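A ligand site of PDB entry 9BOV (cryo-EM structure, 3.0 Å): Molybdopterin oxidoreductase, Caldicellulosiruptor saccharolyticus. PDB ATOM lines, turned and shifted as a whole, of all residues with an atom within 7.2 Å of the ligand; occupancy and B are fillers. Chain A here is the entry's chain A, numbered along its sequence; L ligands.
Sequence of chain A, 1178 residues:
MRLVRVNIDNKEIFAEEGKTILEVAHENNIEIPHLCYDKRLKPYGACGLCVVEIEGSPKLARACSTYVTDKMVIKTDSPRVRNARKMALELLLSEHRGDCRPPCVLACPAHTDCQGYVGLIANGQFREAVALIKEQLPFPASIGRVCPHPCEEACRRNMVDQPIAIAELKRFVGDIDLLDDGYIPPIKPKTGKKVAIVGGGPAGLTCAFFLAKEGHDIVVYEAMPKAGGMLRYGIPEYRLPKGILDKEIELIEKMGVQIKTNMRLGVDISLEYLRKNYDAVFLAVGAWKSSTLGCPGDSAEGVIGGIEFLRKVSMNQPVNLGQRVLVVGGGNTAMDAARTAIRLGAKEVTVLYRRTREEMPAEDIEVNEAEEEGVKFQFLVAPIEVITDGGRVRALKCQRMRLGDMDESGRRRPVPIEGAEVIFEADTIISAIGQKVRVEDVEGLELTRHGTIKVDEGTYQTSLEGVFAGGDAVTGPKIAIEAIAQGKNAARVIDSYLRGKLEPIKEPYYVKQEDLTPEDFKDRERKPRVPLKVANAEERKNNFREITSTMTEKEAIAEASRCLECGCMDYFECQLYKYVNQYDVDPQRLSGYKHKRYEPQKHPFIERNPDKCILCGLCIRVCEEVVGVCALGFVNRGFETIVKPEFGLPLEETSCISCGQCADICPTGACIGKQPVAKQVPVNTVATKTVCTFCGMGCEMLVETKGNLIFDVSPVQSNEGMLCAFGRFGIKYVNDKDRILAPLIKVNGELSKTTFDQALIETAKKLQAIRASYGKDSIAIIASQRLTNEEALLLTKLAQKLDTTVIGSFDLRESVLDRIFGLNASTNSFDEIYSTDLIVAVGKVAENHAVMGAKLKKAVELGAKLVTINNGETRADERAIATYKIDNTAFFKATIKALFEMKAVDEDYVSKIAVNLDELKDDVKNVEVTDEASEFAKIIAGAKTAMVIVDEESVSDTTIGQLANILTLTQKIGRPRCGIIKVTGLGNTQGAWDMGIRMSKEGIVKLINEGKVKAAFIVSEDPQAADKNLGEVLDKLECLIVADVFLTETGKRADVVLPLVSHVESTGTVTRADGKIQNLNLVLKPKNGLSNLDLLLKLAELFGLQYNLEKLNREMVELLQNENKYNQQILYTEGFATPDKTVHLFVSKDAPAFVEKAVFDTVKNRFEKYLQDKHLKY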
ATOM      1  N   LEU A  35     -13.191 -18.082  11.225  1.00  0.00           N
ATOM      2  CA  LEU A  35     -12.750 -16.913  11.977  1.00  0.00           C
ATOM      3  C   LEU A  35     -12.906 -17.121  13.470  1.00  0.00           C
ATOM      4  O   LEU A  35     -12.133 -16.570  14.259  1.00  0.00           O
ATOM      5  CB  LEU A  35     -13.515 -15.669  11.527  1.00  0.00           C
ATOM      6  CG  LEU A  35     -13.178 -15.138  10.126  1.00  0.00           C
ATOM      7  CD1 LEU A  35     -14.095 -13.980   9.756  1.00  0.00           C
ATOM      8  CD2 LEU A  35     -11.726 -14.709  10.051  1.00  0.00           C
ATOM      9  N   CYS A  36     -13.892 -17.919  13.876  1.00  0.00           N
ATOM     10  CA  CYS A  36     -14.191 -18.153  15.283  1.00  0.00           C
ATOM     11  C   CYS A  36     -13.923 -19.602  15.699  1.00  0.00           C
ATOM     12  O   CYS A  36     -14.641 -20.171  16.521  1.00  0.00           O
ATOM     13  CB  CYS A  36     -15.639 -17.785  15.600  1.00  0.00           C
ATOM     14  SG  CYS A  36     -16.871 -18.850  14.818  1.00  0.00           S
ATOM     15  N   ARG A 608      -6.395  -2.753  22.590  1.00  0.00           N
ATOM     16  CA  ARG A 608      -7.688  -3.259  22.153  1.00  0.00           C
ATOM     17  C   ARG A 608      -8.441  -2.181  21.388  1.00  0.00           C
ATOM     18  O   ARG A 608      -8.456  -1.013  21.792  1.00  0.00           O
ATOM     19  CB  ARG A 608      -8.519  -3.735  23.337  1.00  0.00           C
ATOM     20  CG  ARG A 608      -7.712  -4.126  24.559  1.00  0.00           C
ATOM     21  CD  ARG A 608      -8.613  -4.529  25.714  1.00  0.00           C
ATOM     22  NE  ARG A 608      -9.257  -5.804  25.457  1.00  0.00           N
ATOM     23  CZ  ARG A 608     -10.517  -5.938  25.074  1.00  0.00           C
ATOM     24  NH1 ARG A 608     -11.309  -4.888  24.905  1.00  0.00           N
ATOM     25  NH2 ARG A 608     -10.995  -7.154  24.837  1.00  0.00           N
ATOM     26  N   ASN A 609      -9.065  -2.572  20.275  1.00  0.00           N
ATOM     27  CA  ASN A 609      -9.759  -1.642  19.394  1.00  0.00           C
ATOM     28  C   ASN A 609     -11.145  -2.207  19.076  1.00  0.00           C
ATOM     29  O   ASN A 609     -11.274  -3.117  18.253  1.00  0.00           O
ATOM     30  CB  ASN A 609      -8.973  -1.416  18.112  1.00  0.00           C
ATOM     31  CG  ASN A 609      -9.591  -0.372  17.211  1.00  0.00           C
ATOM     32  OD1 ASN A 609     -10.621   0.206  17.528  1.00  0.00           O
ATOM     33  ND2 ASN A 609      -8.956  -0.127  16.068  1.00  0.00           N
ATOM     34  N   PRO A 610     -12.196  -1.687  19.722  1.00  0.00           N
ATOM     35  CA  PRO A 610     -13.541  -2.244  19.489  1.00  0.00           C
ATOM     36  C   PRO A 610     -14.038  -2.081  18.064  1.00  0.00           C
ATOM     37  O   PRO A 610     -14.965  -2.794  17.658  1.00  0.00           O
ATOM     38  CB  PRO A 610     -14.429  -1.462  20.468  1.00  0.00           C
ATOM     39  CG  PRO A 610     -13.487  -0.887  21.462  1.00  0.00           C
ATOM     40  CD  PRO A 610     -12.207  -0.626  20.739  1.00  0.00           C
ATOM     41  N   LYS A 612     -12.622  -2.789  15.230  1.00  0.00           N
ATOM     42  CA  LYS A 612     -12.212  -3.868  14.343  1.00  0.00           C
ATOM     43  C   LYS A 612     -12.556  -5.243  14.907  1.00  0.00           C
ATOM     44  O   LYS A 612     -11.979  -6.253  14.487  1.00  0.00           O
ATOM     45  CB  LYS A 612     -10.718  -3.776  14.038  1.00  0.00           C
ATOM     46  CG  LYS A 612     -10.302  -2.446  13.461  1.00  0.00           C
ATOM     47  CD  LYS A 612      -8.803  -2.376  13.264  1.00  0.00           C
ATOM     48  CE  LYS A 612      -8.390  -0.994  12.790  1.00  0.00           C
ATOM     49  NZ  LYS A 612      -6.917  -0.843  12.743  1.00  0.00           N
ATOM     50  N   CYS A 613     -13.475  -5.295  15.865  1.00  0.00           N
ATOM     51  CA  CYS A 613     -13.861  -6.547  16.492  1.00  0.00           C
ATOM     52  C   CYS A 613     -15.011  -7.184  15.718  1.00  0.00           C
ATOM     53  O   CYS A 613     -16.046  -6.549  15.518  1.00  0.00           O
ATOM     54  CB  CYS A 613     -14.265  -6.319  17.944  1.00  0.00           C
ATOM     55  SG  CYS A 613     -14.836  -7.784  18.808  1.00  0.00           S
ATOM     56  N   ILE A 614     -14.817  -8.434  15.296  1.00  0.00           N
ATOM     57  CA  ILE A 614     -15.865  -9.188  14.625  1.00  0.00           C
ATOM     58  C   ILE A 614     -16.647 -10.059  15.596  1.00  0.00           C
ATOM     59  O   ILE A 614     -17.449 -10.887  15.180  1.00  0.00           O
ATOM     60  CB  ILE A 614     -15.298 -10.024  13.470  1.00  0.00           C
ATOM     61  CG1 ILE A 614     -14.328 -11.078  14.000  1.00  0.00           C
ATOM     62  CG2 ILE A 614     -14.607  -9.132  12.456  1.00  0.00           C
ATOM     63  CD1 ILE A 614     -14.063 -12.199  13.032  1.00  0.00           C
ATOM     64  N   LEU A 615     -16.409  -9.890  16.900  1.00  0.00           N
ATOM     65  CA  LEU A 615     -17.173 -10.559  17.947  1.00  0.00           C
ATOM     66  C   LEU A 615     -17.184 -12.079  17.772  1.00  0.00           C
ATOM     67  O   LEU A 615     -18.217 -12.730  17.926  1.00  0.00           O
ATOM     68  CB  LEU A 615     -18.590 -10.004  18.032  1.00  0.00           C
ATOM     69  CG  LEU A 615     -18.704  -8.684  18.781  1.00  0.00           C
ATOM     70  CD1 LEU A 615     -20.032  -8.011  18.507  1.00  0.00           C
ATOM     71  CD2 LEU A 615     -18.526  -8.906  20.261  1.00  0.00           C
ATOM     72  N   CYS A 616     -16.018 -12.633  17.435  1.00  0.00           N
ATOM     73  CA  CYS A 616     -15.868 -14.074  17.378  1.00  0.00           C
ATOM     74  C   CYS A 616     -15.780 -14.703  18.758  1.00  0.00           C
ATOM     75  O   CYS A 616     -15.959 -15.919  18.889  1.00  0.00           O
ATOM     76  CB  CYS A 616     -14.647 -14.443  16.554  1.00  0.00           C
ATOM     77  SG  CYS A 616     -13.107 -13.732  17.145  1.00  0.00           S
ATOM     78  N   GLY A 617     -15.497 -13.911  19.783  1.00  0.00           N
ATOM     79  CA  GLY A 617     -15.412 -14.418  21.140  1.00  0.00           C
ATOM     80  C   GLY A 617     -14.143 -15.167  21.470  1.00  0.00           C
ATOM     81  O   GLY A 617     -14.035 -15.708  22.567  1.00  0.00           O
ATOM     82  N   LEU A 618     -13.180 -15.198  20.554  1.00  0.00           N
ATOM     83  CA  LEU A 618     -11.981 -16.008  20.748  1.00  0.00           C
ATOM     84  C   LEU A 618     -11.176 -15.540  21.948  1.00  0.00           C
ATOM     85  O   LEU A 618     -10.651 -16.365  22.701  1.00  0.00           O
ATOM     86  CB  LEU A 618     -11.124 -15.990  19.484  1.00  0.00           C
ATOM     87  CG  LEU A 618     -11.497 -16.979  18.385  1.00  0.00           C
ATOM     88  CD1 LEU A 618     -10.637 -16.764  17.165  1.00  0.00           C
ATOM     89  CD2 LEU A 618     -11.366 -18.405  18.877  1.00  0.00           C
ATOM     90  N   CYS A 619     -11.055 -14.228  22.126  1.00  0.00           N
ATOM     91  CA  CYS A 619     -10.299 -13.714  23.266  1.00  0.00           C
ATOM     92  C   CYS A 619     -10.937 -14.117  24.582  1.00  0.00           C
ATOM     93  O   CYS A 619     -10.247 -14.550  25.522  1.00  0.00           O
ATOM     94  CB  CYS A 619     -10.176 -12.194  23.175  1.00  0.00           C
ATOM     95  SG  CYS A 619     -11.735 -11.332  22.952  1.00  0.00           S
ATOM     96  N   ILE A 620     -12.268 -13.984  24.686  1.00  0.00           N
ATOM     97  CA  ILE A 620     -12.971 -14.378  25.904  1.00  0.00           C
ATOM     98  C   ILE A 620     -12.822 -15.870  26.151  1.00  0.00           C
ATOM     99  O   ILE A 620     -12.525 -16.308  27.276  1.00  0.00           O
ATOM    100  CB  ILE A 620     -14.447 -13.964  25.813  1.00  0.00           C
ATOM    101  CG1 ILE A 620     -14.575 -12.459  25.641  1.00  0.00           C
ATOM    102  CG2 ILE A 620     -15.200 -14.427  27.042  1.00  0.00           C
ATOM    103  CD1 ILE A 620     -15.841 -12.053  24.956  1.00  0.00           C
ATOM    104  N   LEU A 632     -11.827 -11.100  30.557  1.00  0.00           N
ATOM    105  CA  LEU A 632     -12.611 -10.476  29.494  1.00  0.00           C
ATOM    106  C   LEU A 632     -14.020 -11.046  29.496  1.00  0.00           C
ATOM    107  O   LEU A 632     -14.259 -12.161  29.982  1.00  0.00           O
ATOM    108  CB  LEU A 632     -11.976 -10.701  28.118  1.00  0.00           C
ATOM    109  CG  LEU A 632     -10.537 -10.242  27.903  1.00  0.00           C
ATOM    110  CD1 LEU A 632     -10.020 -10.777  26.588  1.00  0.00           C
ATOM    111  CD2 LEU A 632     -10.453  -8.732  27.934  1.00  0.00           C
ATOM    112  N   PHE A 634     -18.238 -10.468  27.441  1.00  0.00           N
ATOM    113  CA  PHE A 634     -19.174  -9.724  26.620  1.00  0.00           C
ATOM    114  C   PHE A 634     -19.894  -8.676  27.462  1.00  0.00           C
ATOM    115  O   PHE A 634     -20.089  -8.841  28.663  1.00  0.00           O
ATOM    116  CB  PHE A 634     -20.181 -10.661  25.978  1.00  0.00           C
ATOM    117  CG  PHE A 634     -19.625 -11.447  24.818  1.00  0.00           C
ATOM    118  CD1 PHE A 634     -19.178 -10.808  23.689  1.00  0.00           C
ATOM    119  CD2 PHE A 634     -19.555 -12.820  24.889  1.00  0.00           C
ATOM    120  CE1 PHE A 634     -18.668 -11.531  22.629  1.00  0.00           C
ATOM    121  CE2 PHE A 634     -19.039 -13.547  23.836  1.00  0.00           C
ATOM    122  CZ  PHE A 634     -18.598 -12.905  22.700  1.00  0.00           C
ATOM    123  N   VAL A 643     -16.652  -6.501  23.557  1.00  0.00           N
ATOM    124  CA  VAL A 643     -15.791  -7.262  24.453  1.00  0.00           C
ATOM    125  C   VAL A 643     -15.054  -6.291  25.362  1.00  0.00           C
ATOM    126  O   VAL A 643     -14.346  -5.391  24.894  1.00  0.00           O
ATOM    127  CB  VAL A 643     -14.795  -8.123  23.664  1.00  0.00           C
ATOM    128  CG1 VAL A 643     -13.855  -8.839  24.609  1.00  0.00           C
ATOM    129  CG2 VAL A 643     -15.546  -9.113  22.782  1.00  0.00           C
ATOM    130  N   CYS A 662      -5.015 -13.393  24.248  1.00  0.00           N
ATOM    131  CA  CYS A 662      -6.089 -12.719  23.519  1.00  0.00           C
ATOM    132  C   CYS A 662      -5.567 -12.011  22.290  1.00  0.00           C
ATOM    133  O   CYS A 662      -6.225 -11.997  21.246  1.00  0.00           O
ATOM    134  CB  CYS A 662      -6.810 -11.737  24.447  1.00  0.00           C
ATOM    135  SG  CYS A 662      -5.716 -10.618  25.353  1.00  0.00           S
ATOM    136  N   ALA A 663      -4.378 -11.408  22.377  1.00  0.00           N
ATOM    137  CA  ALA A 663      -3.780 -10.764  21.220  1.00  0.00           C
ATOM    138  C   ALA A 663      -3.323 -11.785  20.192  1.00  0.00           C
ATOM    139  O   ALA A 663      -3.399 -11.544  18.991  1.00  0.00           O
ATOM    140  CB  ALA A 663      -2.617  -9.885  21.655  1.00  0.00           C
ATOM    141  N   ILE A 665      -4.680 -14.737  19.647  1.00  0.00           N
ATOM    142  CA  ILE A 665      -5.803 -15.468  19.060  1.00  0.00           C
ATOM    143  C   ILE A 665      -6.732 -14.568  18.256  1.00  0.00           C
ATOM    144  O   ILE A 665      -7.566 -15.090  17.489  1.00  0.00           O
ATOM    145  CB  ILE A 665      -6.610 -16.206  20.155  1.00  0.00           C
ATOM    146  CG1 ILE A 665      -7.265 -17.454  19.576  1.00  0.00           C
ATOM    147  CG2 ILE A 665      -7.640 -15.300  20.775  1.00  0.00           C
ATOM    148  CD1 ILE A 665      -7.950 -18.310  20.607  1.00  0.00           C
ATOM    149  N   CYS A 666      -6.629 -13.257  18.377  1.00  0.00           N
ATOM    150  CA  CYS A 666      -7.525 -12.361  17.656  1.00  0.00           C
ATOM    151  C   CYS A 666      -7.255 -12.431  16.163  1.00  0.00           C
ATOM    152  O   CYS A 666      -6.094 -12.365  15.750  1.00  0.00           O
ATOM    153  CB  CYS A 666      -7.378 -10.934  18.158  1.00  0.00           C
ATOM    154  SG  CYS A 666      -8.557  -9.778  17.445  1.00  0.00           S
ATOM    155  N   PRO A 667      -8.283 -12.566  15.327  1.00  0.00           N
ATOM    156  CA  PRO A 667      -8.046 -12.668  13.882  1.00  0.00           C
ATOM    157  C   PRO A 667      -7.975 -11.329  13.157  1.00  0.00           C
ATOM    158  O   PRO A 667      -7.292 -11.227  12.130  1.00  0.00           O
ATOM    159  CB  PRO A 667      -9.260 -13.484  13.398  1.00  0.00           C
ATOM    160  CG  PRO A 667     -10.331 -13.149  14.367  1.00  0.00           C
ATOM    161  CD  PRO A 667      -9.671 -12.884  15.682  1.00  0.00           C
ATOM    162  N   THR A 668      -8.642 -10.302  13.669  1.00  0.00           N
ATOM    163  CA  THR A 668      -8.857  -9.071  12.932  1.00  0.00           C
ATOM    164  C   THR A 668      -8.284  -7.850  13.655  1.00  0.00           C
ATOM    165  O   THR A 668      -8.924  -6.802  13.730  1.00  0.00           O
ATOM    166  CB  THR A 668     -10.342  -8.839  12.658  1.00  0.00           C
ATOM    167  OG1 THR A 668     -10.942  -8.226  13.805  1.00  0.00           O
ATOM    168  CG2 THR A 668     -11.047 -10.156  12.367  1.00  0.00           C
ATOM    169  N   GLY A 669      -7.090  -7.985  14.207  1.00  0.00           N
ATOM    170  CA  GLY A 669      -6.346  -6.839  14.715  1.00  0.00           C
ATOM    171  C   GLY A 669      -7.049  -5.934  15.709  1.00  0.00           C
ATOM    172  O   GLY A 669      -6.571  -4.839  15.988  1.00  0.00           O
ATOM    173  N   ALA A 670      -8.185  -6.374  16.245  1.00  0.00           N
ATOM    174  CA  ALA A 670      -8.848  -5.593  17.289  1.00  0.00           C
ATOM    175  C   ALA A 670      -8.041  -5.625  18.583  1.00  0.00           C
ATOM    176  O   ALA A 670      -7.861  -4.589  19.234  1.00  0.00           O
ATOM    177  CB  ALA A 670     -10.259  -6.122  17.525  1.00  0.00           C
ATOM    178  N   CYS A 671      -7.551  -6.792  18.955  1.00  0.00           N
ATOM    179  CA  CYS A 671      -6.618  -6.966  20.057  1.00  0.00           C
ATOM    180  C   CYS A 671      -5.249  -7.275  19.473  1.00  0.00           C
ATOM    181  O   CYS A 671      -5.092  -8.243  18.718  1.00  0.00           O
ATOM    182  CB  CYS A 671      -7.076  -8.080  20.999  1.00  0.00           C
ATOM    183  SG  CYS A 671      -6.691  -7.809  22.736  1.00  0.00           S
HETATM  184 FE1  LIG L   1     -11.869 -10.804  20.759  1.00  0.00          FE
HETATM  185 FE2  LIG L   1     -12.592 -11.889  18.359  1.00  0.00          FE
HETATM  186 FE3  LIG L   1     -10.542 -10.089  18.479  1.00  0.00          FE
HETATM  187 FE4  LIG L   1     -13.124  -9.266  18.885  1.00  0.00          FE
HETATM  188  S1  LIG L   1     -12.248 -10.126  16.968  1.00  0.00           S
HETATM  189  S2  LIG L   1     -11.294  -8.701  20.126  1.00  0.00           S
HETATM  190  S3  LIG L   1     -13.984 -11.079  19.959  1.00  0.00           S
HETATM  191  S4  LIG L   1     -10.603 -12.158  19.434  1.00  0.00           S
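The side-chain sulfur (SG) of Cys 666 is bound to an iron atom (FE3) of the ligand (2.3 Å).
An iron atom (FE2) of the ligand is bound by the side-chain sulfur (SG) of Cys 616, 2.3 Å away.
A sulfur (S1) of the ligand lies close to the backbone NH of Ile 614, 3.5 Å away.
The side-chain sulfur (SG) of Cys 619 is bound to an iron atom (FE1) of the ligand (2.3 Å).
SG of Cys 613 binds FE4 of the ligand (2.3 Å).
A sulfur (S3) of the ligand sits close to the backbone NH (N) of Gly 617, at 3.2 Å.
The backbone NH of Cys 616 lies close to a sulfur (S3) of the ligand.
S4 of the ligand sits close to N of Cys 619.
The side-chain sulfur (SG) of Cys 666 lies close to the backbone NH (N) of Ala 670 (3.6 Å).
The side-chain sulfur of Cys 616 lies close to the backbone NH of Leu 618 (3.7 Å).
The backbone carbonyl oxygen (O) of Ala 670 sits at hydrogen-bond distance from the backbone NH (N) of Asn 609 (2.6 Å).
N of Leu 615 lies close to SG of Cys 613 (3.2 Å).
The backbone carbonyl oxygen (O) of Val 643 is in hydrogen-bond range of the guanidinium group (NH1) of Arg 608 (3.1 Å).
The side-chain sulfur (SG) of Cys 666 sits close to the backbone NH (N) of Cys 671, at 3.5 Å.
Residues that only touch the ligand: Val 643 (3.8 Å), Ala 670 (3.8 Å), Leu 615 (3.8 Å), Leu 618 (3.9 Å), Thr 668 (3.9 Å) and Pro 667 (3.9 Å).
Hydrophobic or aromatic side chains that line the ligand: Ile 614, Leu 618, Val 643, Pro 667 and Ala 670.
12 residues have an atom within 4 Å of the ligand: Cys 613, Ile 614, Leu 615, Cys 616, Gly 617, Leu 618, Cys 619, Val 643, Cys 666, Pro 667, Thr 668 and Ala 670.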
